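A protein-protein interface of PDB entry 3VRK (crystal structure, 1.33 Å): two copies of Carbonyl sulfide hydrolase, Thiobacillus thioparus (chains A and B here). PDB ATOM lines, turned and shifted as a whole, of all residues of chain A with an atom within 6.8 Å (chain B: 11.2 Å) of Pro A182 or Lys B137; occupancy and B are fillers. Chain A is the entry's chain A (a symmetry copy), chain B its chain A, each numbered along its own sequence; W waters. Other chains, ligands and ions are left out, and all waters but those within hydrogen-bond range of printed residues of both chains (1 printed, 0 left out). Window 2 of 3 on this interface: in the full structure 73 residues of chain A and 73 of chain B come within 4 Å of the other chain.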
ATOM      1  N   HIS A  85     -14.617 -35.367   9.963  1.00  0.00           N
ATOM      2  CA  HIS A  85     -14.037 -34.257  10.747  1.00  0.00           C
ATOM      3  C   HIS A  85     -14.136 -34.485  12.245  1.00  0.00           C
ATOM      4  O   HIS A  85     -13.254 -33.982  12.962  1.00  0.00           O
ATOM      5  CB  HIS A  85     -14.695 -32.922  10.406  1.00  0.00           C
ATOM      6  CG  HIS A  85     -14.317 -32.386   9.064  1.00  0.00           C
ATOM      7  ND1 HIS A  85     -13.043 -31.858   8.838  1.00  0.00           N
ATOM      8  CD2 HIS A  85     -14.991 -32.293   7.909  1.00  0.00           C
ATOM      9  CE1 HIS A  85     -12.963 -31.443   7.575  1.00  0.00           C
ATOM     10  NE2 HIS A  85     -14.132 -31.707   7.007  1.00  0.00           N
ATOM     11  N   ILE A 177     -19.824 -35.368  -6.331  1.00  0.00           N
ATOM     12  CA  ILE A 177     -20.297 -34.461  -5.262  1.00  0.00           C
ATOM     13  C   ILE A 177     -19.318 -34.466  -4.115  1.00  0.00           C
ATOM     14  O   ILE A 177     -18.913 -33.435  -3.565  1.00  0.00           O
ATOM     15  CB  ILE A 177     -21.729 -34.854  -4.826  1.00  0.00           C
ATOM     16  CG1 ILE A 177     -22.709 -34.611  -5.973  1.00  0.00           C
ATOM     17  CG2 ILE A 177     -22.080 -34.172  -3.495  1.00  0.00           C
ATOM     18  CD1 ILE A 177     -24.101 -35.116  -5.690  1.00  0.00           C
ATOM     19  N   ILE A 178     -18.892 -35.661  -3.683  1.00  0.00           N
ATOM     20  CA  ILE A 178     -17.989 -35.751  -2.549  1.00  0.00           C
ATOM     21  C   ILE A 178     -16.666 -35.092  -2.886  1.00  0.00           C
ATOM     22  O   ILE A 178     -16.074 -34.412  -2.042  1.00  0.00           O
ATOM     23  CB  ILE A 178     -17.801 -37.271  -2.219  1.00  0.00           C
ATOM     24  CG1 ILE A 178     -19.054 -37.819  -1.566  1.00  0.00           C
ATOM     25  CG2 ILE A 178     -16.549 -37.531  -1.396  1.00  0.00           C
ATOM     26  CD1 ILE A 178     -19.163 -39.330  -1.546  1.00  0.00           C
ATOM     27  N   ASN A 180     -15.947 -32.721  -4.794  1.00  0.00           N
ATOM     28  CA  ASN A 180     -15.965 -31.263  -5.034  1.00  0.00           C
ATOM     29  C   ASN A 180     -16.691 -30.482  -3.966  1.00  0.00           C
ATOM     30  O   ASN A 180     -16.816 -29.261  -4.064  1.00  0.00           O
ATOM     31  CB  ASN A 180     -16.582 -31.017  -6.420  1.00  0.00           C
ATOM     32  CG  ASN A 180     -15.657 -31.595  -7.494  1.00  0.00           C
ATOM     33  OD1 ASN A 180     -14.594 -31.048  -7.756  1.00  0.00           O
ATOM     34  ND2 ASN A 180     -16.016 -32.715  -8.091  1.00  0.00           N
ATOM     35  N   HIS A 181     -17.160 -31.123  -2.897  1.00  0.00           N
ATOM     36  CA  HIS A 181     -17.856 -30.370  -1.829  1.00  0.00           C
ATOM     37  C   HIS A 181     -16.879 -29.518  -1.038  1.00  0.00           C
ATOM     38  O   HIS A 181     -15.807 -30.019  -0.653  1.00  0.00           O
ATOM     39  CB  HIS A 181     -18.634 -31.325  -0.901  1.00  0.00           C
ATOM     40  CG  HIS A 181     -19.537 -30.510   0.005  1.00  0.00           C
ATOM     41  ND1 HIS A 181     -19.123 -29.829   1.133  1.00  0.00           N
ATOM     42  CD2 HIS A 181     -20.868 -30.272  -0.139  1.00  0.00           C
ATOM     43  CE1 HIS A 181     -20.157 -29.212   1.647  1.00  0.00           C
ATOM     44  NE2 HIS A 181     -21.232 -29.453   0.904  1.00  0.00           N
ATOM     45  N   PRO A 182     -17.154 -28.242  -0.765  1.00  0.00           N
ATOM     46  CA  PRO A 182     -16.219 -27.416  -0.003  1.00  0.00           C
ATOM     47  C   PRO A 182     -15.768 -27.928   1.357  1.00  0.00           C
ATOM     48  O   PRO A 182     -14.708 -27.488   1.812  1.00  0.00           O
ATOM     49  CB  PRO A 182     -17.025 -26.112   0.253  1.00  0.00           C
ATOM     50  CG  PRO A 182     -18.156 -26.096  -0.683  1.00  0.00           C
ATOM     51  CD  PRO A 182     -18.333 -27.487  -1.224  1.00  0.00           C
ATOM     52  N   TRP A 183     -16.557 -28.775   2.022  1.00  0.00           N
ATOM     53  CA  TRP A 183     -16.283 -29.161   3.393  1.00  0.00           C
ATOM     54  C   TRP A 183     -15.830 -30.612   3.549  1.00  0.00           C
ATOM     55  O   TRP A 183     -15.760 -31.124   4.689  1.00  0.00           O
ATOM     56  CB  TRP A 183     -17.560 -28.923   4.221  1.00  0.00           C
ATOM     57  CG  TRP A 183     -17.741 -27.473   4.597  1.00  0.00           C
ATOM     58  CD1 TRP A 183     -16.855 -26.443   4.377  1.00  0.00           C
ATOM     59  CD2 TRP A 183     -18.877 -26.925   5.278  1.00  0.00           C
ATOM     60  NE1 TRP A 183     -17.368 -25.265   4.873  1.00  0.00           N
ATOM     61  CE2 TRP A 183     -18.612 -25.541   5.429  1.00  0.00           C
ATOM     62  CE3 TRP A 183     -20.098 -27.429   5.766  1.00  0.00           C
ATOM     63  CZ2 TRP A 183     -19.510 -24.682   6.059  1.00  0.00           C
ATOM     64  CZ3 TRP A 183     -20.987 -26.566   6.384  1.00  0.00           C
ATOM     65  CH2 TRP A 183     -20.688 -25.181   6.517  1.00  0.00           C
ATOM     66  N   LEU A 184     -15.508 -31.267   2.435  1.00  0.00           N
ATOM     67  CA  LEU A 184     -14.873 -32.588   2.497  1.00  0.00           C
ATOM     68  C   LEU A 184     -13.487 -32.513   1.884  1.00  0.00           C
ATOM     69  O   LEU A 184     -13.351 -32.189   0.707  1.00  0.00           O
ATOM     70  CB  LEU A 184     -15.696 -33.665   1.792  1.00  0.00           C
ATOM     71  CG  LEU A 184     -17.026 -33.976   2.512  1.00  0.00           C
ATOM     72  CD1 LEU A 184     -17.823 -34.923   1.618  1.00  0.00           C
ATOM     73  CD2 LEU A 184     -16.840 -34.583   3.886  1.00  0.00           C
ATOM     74  N   PRO A 185     -12.431 -32.785   2.653  1.00  0.00           N
ATOM     75  CA  PRO A 185     -11.058 -32.724   2.153  1.00  0.00           C
ATOM     76  C   PRO A 185     -10.764 -34.036   1.416  1.00  0.00           C
ATOM     77  O   PRO A 185     -10.774 -35.072   2.020  1.00  0.00           O
ATOM     78  CB  PRO A 185     -10.210 -32.563   3.413  1.00  0.00           C
ATOM     79  CG  PRO A 185     -11.004 -33.280   4.443  1.00  0.00           C
ATOM     80  CD  PRO A 185     -12.473 -33.115   4.105  1.00  0.00           C
ATOM     81  N   ASP B 108     -23.073 -24.620  15.442  1.00  0.00           N
ATOM     82  CA  ASP B 108     -22.305 -23.407  15.203  1.00  0.00           C
ATOM     83  C   ASP B 108     -20.806 -23.589  15.372  1.00  0.00           C
ATOM     84  O   ASP B 108     -20.031 -22.992  14.638  1.00  0.00           O
ATOM     85  CB  ASP B 108     -22.784 -22.250  16.115  1.00  0.00           C
ATOM     86  N   LEU B 109     -20.354 -24.396  16.327  1.00  0.00           N
ATOM     87  CA  LEU B 109     -18.949 -24.683  16.450  1.00  0.00           C
ATOM     88  C   LEU B 109     -18.377 -25.356  15.202  1.00  0.00           C
ATOM     89  O   LEU B 109     -17.351 -24.908  14.708  1.00  0.00           O
ATOM     90  CB  LEU B 109     -18.722 -25.608  17.644  1.00  0.00           C
ATOM     91  CG  LEU B 109     -17.256 -25.934  17.905  1.00  0.00           C
ATOM     92  CD1 LEU B 109     -16.515 -24.630  18.147  1.00  0.00           C
ATOM     93  CD2 LEU B 109     -17.160 -26.901  19.075  1.00  0.00           C
ATOM     94  N   LEU B 110     -19.033 -26.415  14.729  1.00  0.00           N
ATOM     95  CA  LEU B 110     -18.533 -27.117  13.558  1.00  0.00           C
ATOM     96  C   LEU B 110     -18.552 -26.220  12.341  1.00  0.00           C
ATOM     97  O   LEU B 110     -17.576 -26.203  11.588  1.00  0.00           O
ATOM     98  CB  LEU B 110     -19.371 -28.384  13.338  1.00  0.00           C
ATOM     99  CG  LEU B 110     -18.881 -29.228  12.120  1.00  0.00           C
ATOM    100  CD1 LEU B 110     -17.390 -29.540  12.157  1.00  0.00           C
ATOM    101  CD2 LEU B 110     -19.689 -30.508  12.045  1.00  0.00           C
ATOM    102  N   ARG B 111     -19.628 -25.458  12.127  1.00  0.00           N
ATOM    103  CA  ARG B 111     -19.705 -24.511  11.018  1.00  0.00           C
ATOM    104  C   ARG B 111     -18.527 -23.536  11.040  1.00  0.00           C
ATOM    105  O   ARG B 111     -17.849 -23.316  10.045  1.00  0.00           O
ATOM    106  CB  ARG B 111     -21.023 -23.738  11.094  1.00  0.00           C
ATOM    107  CG  ARG B 111     -21.573 -23.165   9.824  1.00  0.00           C
ATOM    108  CD  ARG B 111     -23.091 -23.073   9.723  1.00  0.00           C
ATOM    109  NE  ARG B 111     -23.763 -24.336   9.872  1.00  0.00           N
ATOM    110  CZ  ARG B 111     -24.224 -25.119   8.923  1.00  0.00           C
ATOM    111  NH1 ARG B 111     -24.823 -26.270   9.224  1.00  0.00           N
ATOM    112  NH2 ARG B 111     -24.136 -24.818   7.653  1.00  0.00           N
ATOM    113  N   ALA B 112     -18.314 -22.926  12.202  1.00  0.00           N
ATOM    114  CA  ALA B 112     -17.257 -21.917  12.327  1.00  0.00           C
ATOM    115  C   ALA B 112     -15.903 -22.557  12.112  1.00  0.00           C
ATOM    116  O   ALA B 112     -15.024 -21.962  11.475  1.00  0.00           O
ATOM    117  CB  ALA B 112     -17.331 -21.248  13.693  1.00  0.00           C
ATOM    118  N   GLY B 113     -15.702 -23.775  12.627  1.00  0.00           N
ATOM    119  CA  GLY B 113     -14.418 -24.464  12.402  1.00  0.00           C
ATOM    120  C   GLY B 113     -14.202 -24.721  10.920  1.00  0.00           C
ATOM    121  O   GLY B 113     -13.108 -24.506  10.346  1.00  0.00           O
ATOM    122  N   LEU B 114     -15.262 -25.193  10.238  1.00  0.00           N
ATOM    123  CA  LEU B 114     -15.120 -25.429   8.797  1.00  0.00           C
ATOM    124  C   LEU B 114     -14.861 -24.152   8.007  1.00  0.00           C
ATOM    125  O   LEU B 114     -14.058 -24.140   7.058  1.00  0.00           O
ATOM    126  CB  LEU B 114     -16.352 -26.175   8.274  1.00  0.00           C
ATOM    127  CG  LEU B 114     -16.435 -27.629   8.767  1.00  0.00           C
ATOM    128  CD1 LEU B 114     -17.877 -28.125   8.589  1.00  0.00           C
ATOM    129  CD2 LEU B 114     -15.455 -28.570   8.073  1.00  0.00           C
ATOM    130  N   GLU B 115     -15.535 -23.071   8.388  1.00  0.00           N
ATOM    131  CA  GLU B 115     -15.371 -21.751   7.764  1.00  0.00           C
ATOM    132  C   GLU B 115     -13.969 -21.186   7.890  1.00  0.00           C
ATOM    133  O   GLU B 115     -13.503 -20.378   7.060  1.00  0.00           O
ATOM    134  CB  GLU B 115     -16.345 -20.761   8.419  1.00  0.00           C
ATOM    135  CG  GLU B 115     -17.775 -20.915   7.926  1.00  0.00           C
ATOM    136  CD  GLU B 115     -18.755 -20.137   8.804  1.00  0.00           C
ATOM    137  OE1 GLU B 115     -18.353 -19.446   9.741  1.00  0.00           O
ATOM    138  OE2 GLU B 115     -19.981 -20.219   8.553  1.00  0.00           O
ATOM    139  N   GLY B 116     -13.269 -21.598   8.966  1.00  0.00           N
ATOM    140  CA  GLY B 116     -11.950 -21.099   9.204  1.00  0.00           C
ATOM    141  C   GLY B 116     -11.720 -20.293  10.446  1.00  0.00           C
ATOM    142  O   GLY B 116     -10.613 -19.753  10.609  1.00  0.00           O
ATOM    143  N   ASP B 117     -12.693 -20.162  11.334  1.00  0.00           N
ATOM    144  CA  ASP B 117     -12.397 -19.531  12.640  1.00  0.00           C
ATOM    145  C   ASP B 117     -11.295 -20.297  13.369  1.00  0.00           C
ATOM    146  O   ASP B 117     -11.467 -21.484  13.700  1.00  0.00           O
ATOM    147  CB  ASP B 117     -13.709 -19.471  13.423  1.00  0.00           C
ATOM    148  CG  ASP B 117     -13.600 -18.706  14.710  1.00  0.00           C
ATOM    149  OD1 ASP B 117     -13.737 -17.469  14.682  1.00  0.00           O
ATOM    150  OD2 ASP B 117     -13.366 -19.285  15.771  1.00  0.00           O
ATOM    151  N   ALA B 118     -10.131 -19.709  13.641  1.00  0.00           N
ATOM    152  CA  ALA B 118      -9.028 -20.475  14.224  1.00  0.00           C
ATOM    153  C   ALA B 118      -9.411 -20.967  15.610  1.00  0.00           C
ATOM    154  O   ALA B 118      -9.075 -22.070  16.006  1.00  0.00           O
ATOM    155  CB  ALA B 118      -7.735 -19.669  14.232  1.00  0.00           C
ATOM    156  N   GLU B 121     -11.635 -24.028  15.232  1.00  0.00           N
ATOM    157  CA  GLU B 121     -10.806 -25.127  14.718  1.00  0.00           C
ATOM    158  C   GLU B 121     -10.051 -25.835  15.847  1.00  0.00           C
ATOM    159  O   GLU B 121      -9.991 -27.073  15.963  1.00  0.00           O
ATOM    160  CB  GLU B 121      -9.838 -24.561  13.665  1.00  0.00           C
ATOM    161  CG  GLU B 121      -8.855 -25.580  13.091  1.00  0.00           C
ATOM    162  CD  GLU B 121      -7.850 -24.981  12.129  1.00  0.00           C
ATOM    163  OE1 GLU B 121      -7.221 -23.952  12.455  1.00  0.00           O
ATOM    164  OE2 GLU B 121      -7.664 -25.540  11.016  1.00  0.00           O
ATOM    165  N   PHE B 132      -8.347 -31.811  13.743  1.00  0.00           N
ATOM    166  CA  PHE B 132      -9.322 -31.169  12.884  1.00  0.00           C
ATOM    167  C   PHE B 132      -8.626 -30.039  12.123  1.00  0.00           C
ATOM    168  O   PHE B 132      -7.915 -29.226  12.725  1.00  0.00           O
ATOM    169  CB  PHE B 132     -10.527 -30.663  13.693  1.00  0.00           C
ATOM    170  CG  PHE B 132     -11.451 -29.788  12.869  1.00  0.00           C
ATOM    171  CD1 PHE B 132     -12.450 -30.343  12.093  1.00  0.00           C
ATOM    172  CD2 PHE B 132     -11.337 -28.391  12.850  1.00  0.00           C
ATOM    173  CE1 PHE B 132     -13.290 -29.566  11.298  1.00  0.00           C
ATOM    174  CE2 PHE B 132     -12.129 -27.616  12.031  1.00  0.00           C
ATOM    175  CZ  PHE B 132     -13.120 -28.202  11.270  1.00  0.00           C
ATOM    176  N   VAL B 133      -8.901 -29.966  10.826  1.00  0.00           N
ATOM    177  CA  VAL B 133      -8.357 -28.908   9.986  1.00  0.00           C
ATOM    178  C   VAL B 133      -9.502 -28.193   9.288  1.00  0.00           C
ATOM    179  O   VAL B 133     -10.304 -28.855   8.592  1.00  0.00           O
ATOM    180  CB  VAL B 133      -7.350 -29.548   8.989  1.00  0.00           C
ATOM    181  CG1 VAL B 133      -6.886 -28.484   7.991  1.00  0.00           C
ATOM    182  CG2 VAL B 133      -6.210 -30.181   9.761  1.00  0.00           C
ATOM    183  N   SER B 134      -9.620 -26.885   9.442  1.00  0.00           N
ATOM    184  CA  SER B 134     -10.646 -26.085   8.758  1.00  0.00           C
ATOM    185  C   SER B 134     -10.606 -26.238   7.237  1.00  0.00           C
ATOM    186  O   SER B 134      -9.511 -26.378   6.641  1.00  0.00           O
ATOM    187  CB  SER B 134     -10.491 -24.590   9.077  1.00  0.00           C
ATOM    188  OG  SER B 134     -10.703 -24.305  10.472  1.00  0.00           O
ATOM    189  N   ALA B 135     -11.780 -26.193   6.588  1.00  0.00           N
ATOM    190  CA  ALA B 135     -11.822 -26.084   5.135  1.00  0.00           C
ATOM    191  C   ALA B 135     -11.410 -24.702   4.649  1.00  0.00           C
ATOM    192  O   ALA B 135     -10.936 -24.535   3.515  1.00  0.00           O
ATOM    193  CB  ALA B 135     -13.244 -26.402   4.678  1.00  0.00           C
ATOM    194  N   GLY B 136     -11.575 -23.685   5.492  1.00  0.00           N
ATOM    195  CA  GLY B 136     -11.295 -22.305   5.160  1.00  0.00           C
ATOM    196  C   GLY B 136     -12.239 -21.641   4.177  1.00  0.00           C
ATOM    197  O   GLY B 136     -11.861 -20.676   3.513  1.00  0.00           O
ATOM    198  N   LYS B 137     -13.477 -22.123   4.065  1.00  0.00           N
ATOM    199  CA  LYS B 137     -14.495 -21.536   3.223  1.00  0.00           C
ATOM    200  C   LYS B 137     -15.854 -21.852   3.815  1.00  0.00           C
ATOM    201  O   LYS B 137     -16.019 -22.822   4.543  1.00  0.00           O
ATOM    202  CB  LYS B 137     -14.424 -22.128   1.826  1.00  0.00           C
ATOM    203  CG  LYS B 137     -14.449 -23.650   1.905  1.00  0.00           C
ATOM    204  CD  LYS B 137     -14.106 -24.127   0.485  1.00  0.00           C
ATOM    205  CE  LYS B 137     -12.664 -23.691   0.253  1.00  0.00           C
ATOM    206  NZ  LYS B 137     -12.032 -24.650  -0.697  1.00  0.00           N
ATOM    207  N   ALA B 138     -16.831 -21.010   3.489  1.00  0.00           N
ATOM    208  CA  ALA B 138     -18.204 -21.204   3.904  1.00  0.00           C
ATOM    209  C   ALA B 138     -18.962 -22.047   2.888  1.00  0.00           C
ATOM    210  O   ALA B 138     -18.600 -22.124   1.720  1.00  0.00           O
ATOM    211  CB  ALA B 138     -18.833 -19.838   4.092  1.00  0.00           C
ATOM    212  N   SER B 139     -20.028 -22.675   3.402  1.00  0.00           N
ATOM    213  CA  SER B 139     -20.934 -23.460   2.574  1.00  0.00           C
ATOM    214  C   SER B 139     -22.390 -23.223   3.004  1.00  0.00           C
ATOM    215  O   SER B 139     -22.600 -23.073   4.217  1.00  0.00           O
ATOM    216  CB  SER B 139     -20.615 -24.951   2.724  1.00  0.00           C
ATOM    217  OG  SER B 139     -21.348 -25.727   1.774  1.00  0.00           O
ATOM    218  N   ALA B 140     -23.319 -23.187   2.081  1.00  0.00           N
ATOM    219  CA  ALA B 140     -24.745 -23.127   2.421  1.00  0.00           C
ATOM    220  C   ALA B 140     -25.251 -24.481   2.885  1.00  0.00           C
ATOM    221  O   ALA B 140     -26.242 -24.600   3.605  1.00  0.00           O
ATOM    222  CB  ALA B 140     -25.560 -22.694   1.203  1.00  0.00           C
ATOM    223  N   SER B 141     -24.579 -25.559   2.456  1.00  0.00           N
ATOM    224  CA  SER B 141     -25.117 -26.892   2.728  1.00  0.00           C
ATOM    225  C   SER B 141     -24.018 -27.759   3.333  1.00  0.00           C
ATOM    226  O   SER B 141     -22.855 -27.619   2.915  1.00  0.00           O
ATOM    227  CB  SER B 141     -25.781 -27.368   1.442  1.00  0.00           C
ATOM    228  OG  SER B 141     -26.781 -26.395   1.063  1.00  0.00           O
ATOM    229  N   PRO B 142     -24.325 -28.607   4.282  1.00  0.00           N
ATOM    230  CA  PRO B 142     -25.659 -28.807   4.871  1.00  0.00           C
ATOM    231  C   PRO B 142     -26.057 -27.613   5.762  1.00  0.00           C
ATOM    232  O   PRO B 142     -25.191 -26.996   6.404  1.00  0.00           O
ATOM    233  CB  PRO B 142     -25.518 -30.044   5.742  1.00  0.00           C
ATOM    234  CG  PRO B 142     -24.087 -30.096   6.082  1.00  0.00           C
ATOM    235  CD  PRO B 142     -23.319 -29.530   4.898  1.00  0.00           C
ATOM    236  N   PHE B 145     -26.448 -29.280  11.110  1.00  0.00           N
ATOM    237  CA  PHE B 145     -25.825 -30.580  11.443  1.00  0.00           C
ATOM    238  C   PHE B 145     -26.714 -31.396  12.346  1.00  0.00           C
ATOM    239  O   PHE B 145     -26.514 -32.630  12.432  1.00  0.00           O
ATOM    240  CB  PHE B 145     -24.429 -30.389  12.082  1.00  0.00           C
ATOM    241  CG  PHE B 145     -23.408 -29.940  11.041  1.00  0.00           C
ATOM    242  CD1 PHE B 145     -22.924 -30.883  10.153  1.00  0.00           C
ATOM    243  CD2 PHE B 145     -22.972 -28.628  10.921  1.00  0.00           C
ATOM    244  CE1 PHE B 145     -22.041 -30.535   9.158  1.00  0.00           C
ATOM    245  CE2 PHE B 145     -22.076 -28.281   9.930  1.00  0.00           C
ATOM    246  CZ  PHE B 145     -21.599 -29.232   9.040  1.00  0.00           C
HETATM  247  O   HOH W   1     -10.474 -32.194   9.911  1.00  0.00           O
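A ring nitrogen (NE2) of His A181 sits at hydrogen-bond distance from the backbone carbonyl oxygen of Ser B141 (3.2 Å).
The backbone carbonyl oxygen (O) of Lys B137 sits at hydrogen-bond distance from the indole nitrogen (NE1) of Trp A183 (2.8 Å).
O of Leu B114 is in hydrogen-bond range of N of Ala B135, at 3.1 Å.
ND1 of His A181 lies within hydrogen-bond range of N of Trp A183 (2.9 Å).
The backbone carbonyl oxygen (O) of Glu B115 sits at hydrogen-bond distance from the backbone NH (N) of Lys B137 (3.5 Å).
The backbone carbonyl oxygen (O) of Trp A183 lies within hydrogen-bond range of a ring nitrogen (NE2) of His A85, 2.9 Å away.
The backbone carbonyl oxygen (O) of Pro B142 sits at hydrogen-bond distance from the guanidinium group (NH2) of Arg B111, at 2.7 Å.
The backbone carbonyl oxygen (O) of Leu B114 sits at hydrogen-bond distance from the backbone NH (N) of Gly B136.
Among the printed residues, merely in contact across the chains: His A85 with Leu B114, His A85 with Phe B132, His A85 with Val B133, His A181 with Ser B139, Pro A182 with Ala B135, Pro A182 with Lys B137, Trp A183 with Arg B111, Trp A183 with Leu B114, Trp A183 with Ala B135, Trp A183 with Ser B139, Trp A183 with Ser B141, Trp A183 with Pro B142 and Trp A183 with Phe B145.
Pro A182 touches just these residues of chain B: Ala B135 and Lys B137.
Lys B137 touches just these residues of chain A: Pro A182 and Trp A183.
Of the printed residues of chain A, Phe B132 touches His A85.
Of the printed residues of chain A, Val B133 touches His A85.
Pro A185 touches none of the printed residues of chain B.
Of the 24 printed residues of chain B, 10 touch a printed residue of chain A.
Of the 9 printed residues of chain A, 4 touch a printed residue of chain B.
Printed residues of chain A that touch a printed residue of chain B: His A85, His A181, Pro A182 and Trp A183.
Hydrophobic or aromatic side chains of chain A that line the printed part of chain B: His A85, His A181, Pro A182 and Trp A183.
Among the printed residues, no Asp or Glu carboxylate lies within 4 Å of a Lys or Arg side-chain nitrogen of the other chain.
No position is printed for both chains.
Of the 15 pairs that touch across the chains among the printed residues, none has its exchanged pair printed and touching as well.
Water W1 bridges ND1 of His A85 and N of Val B133.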
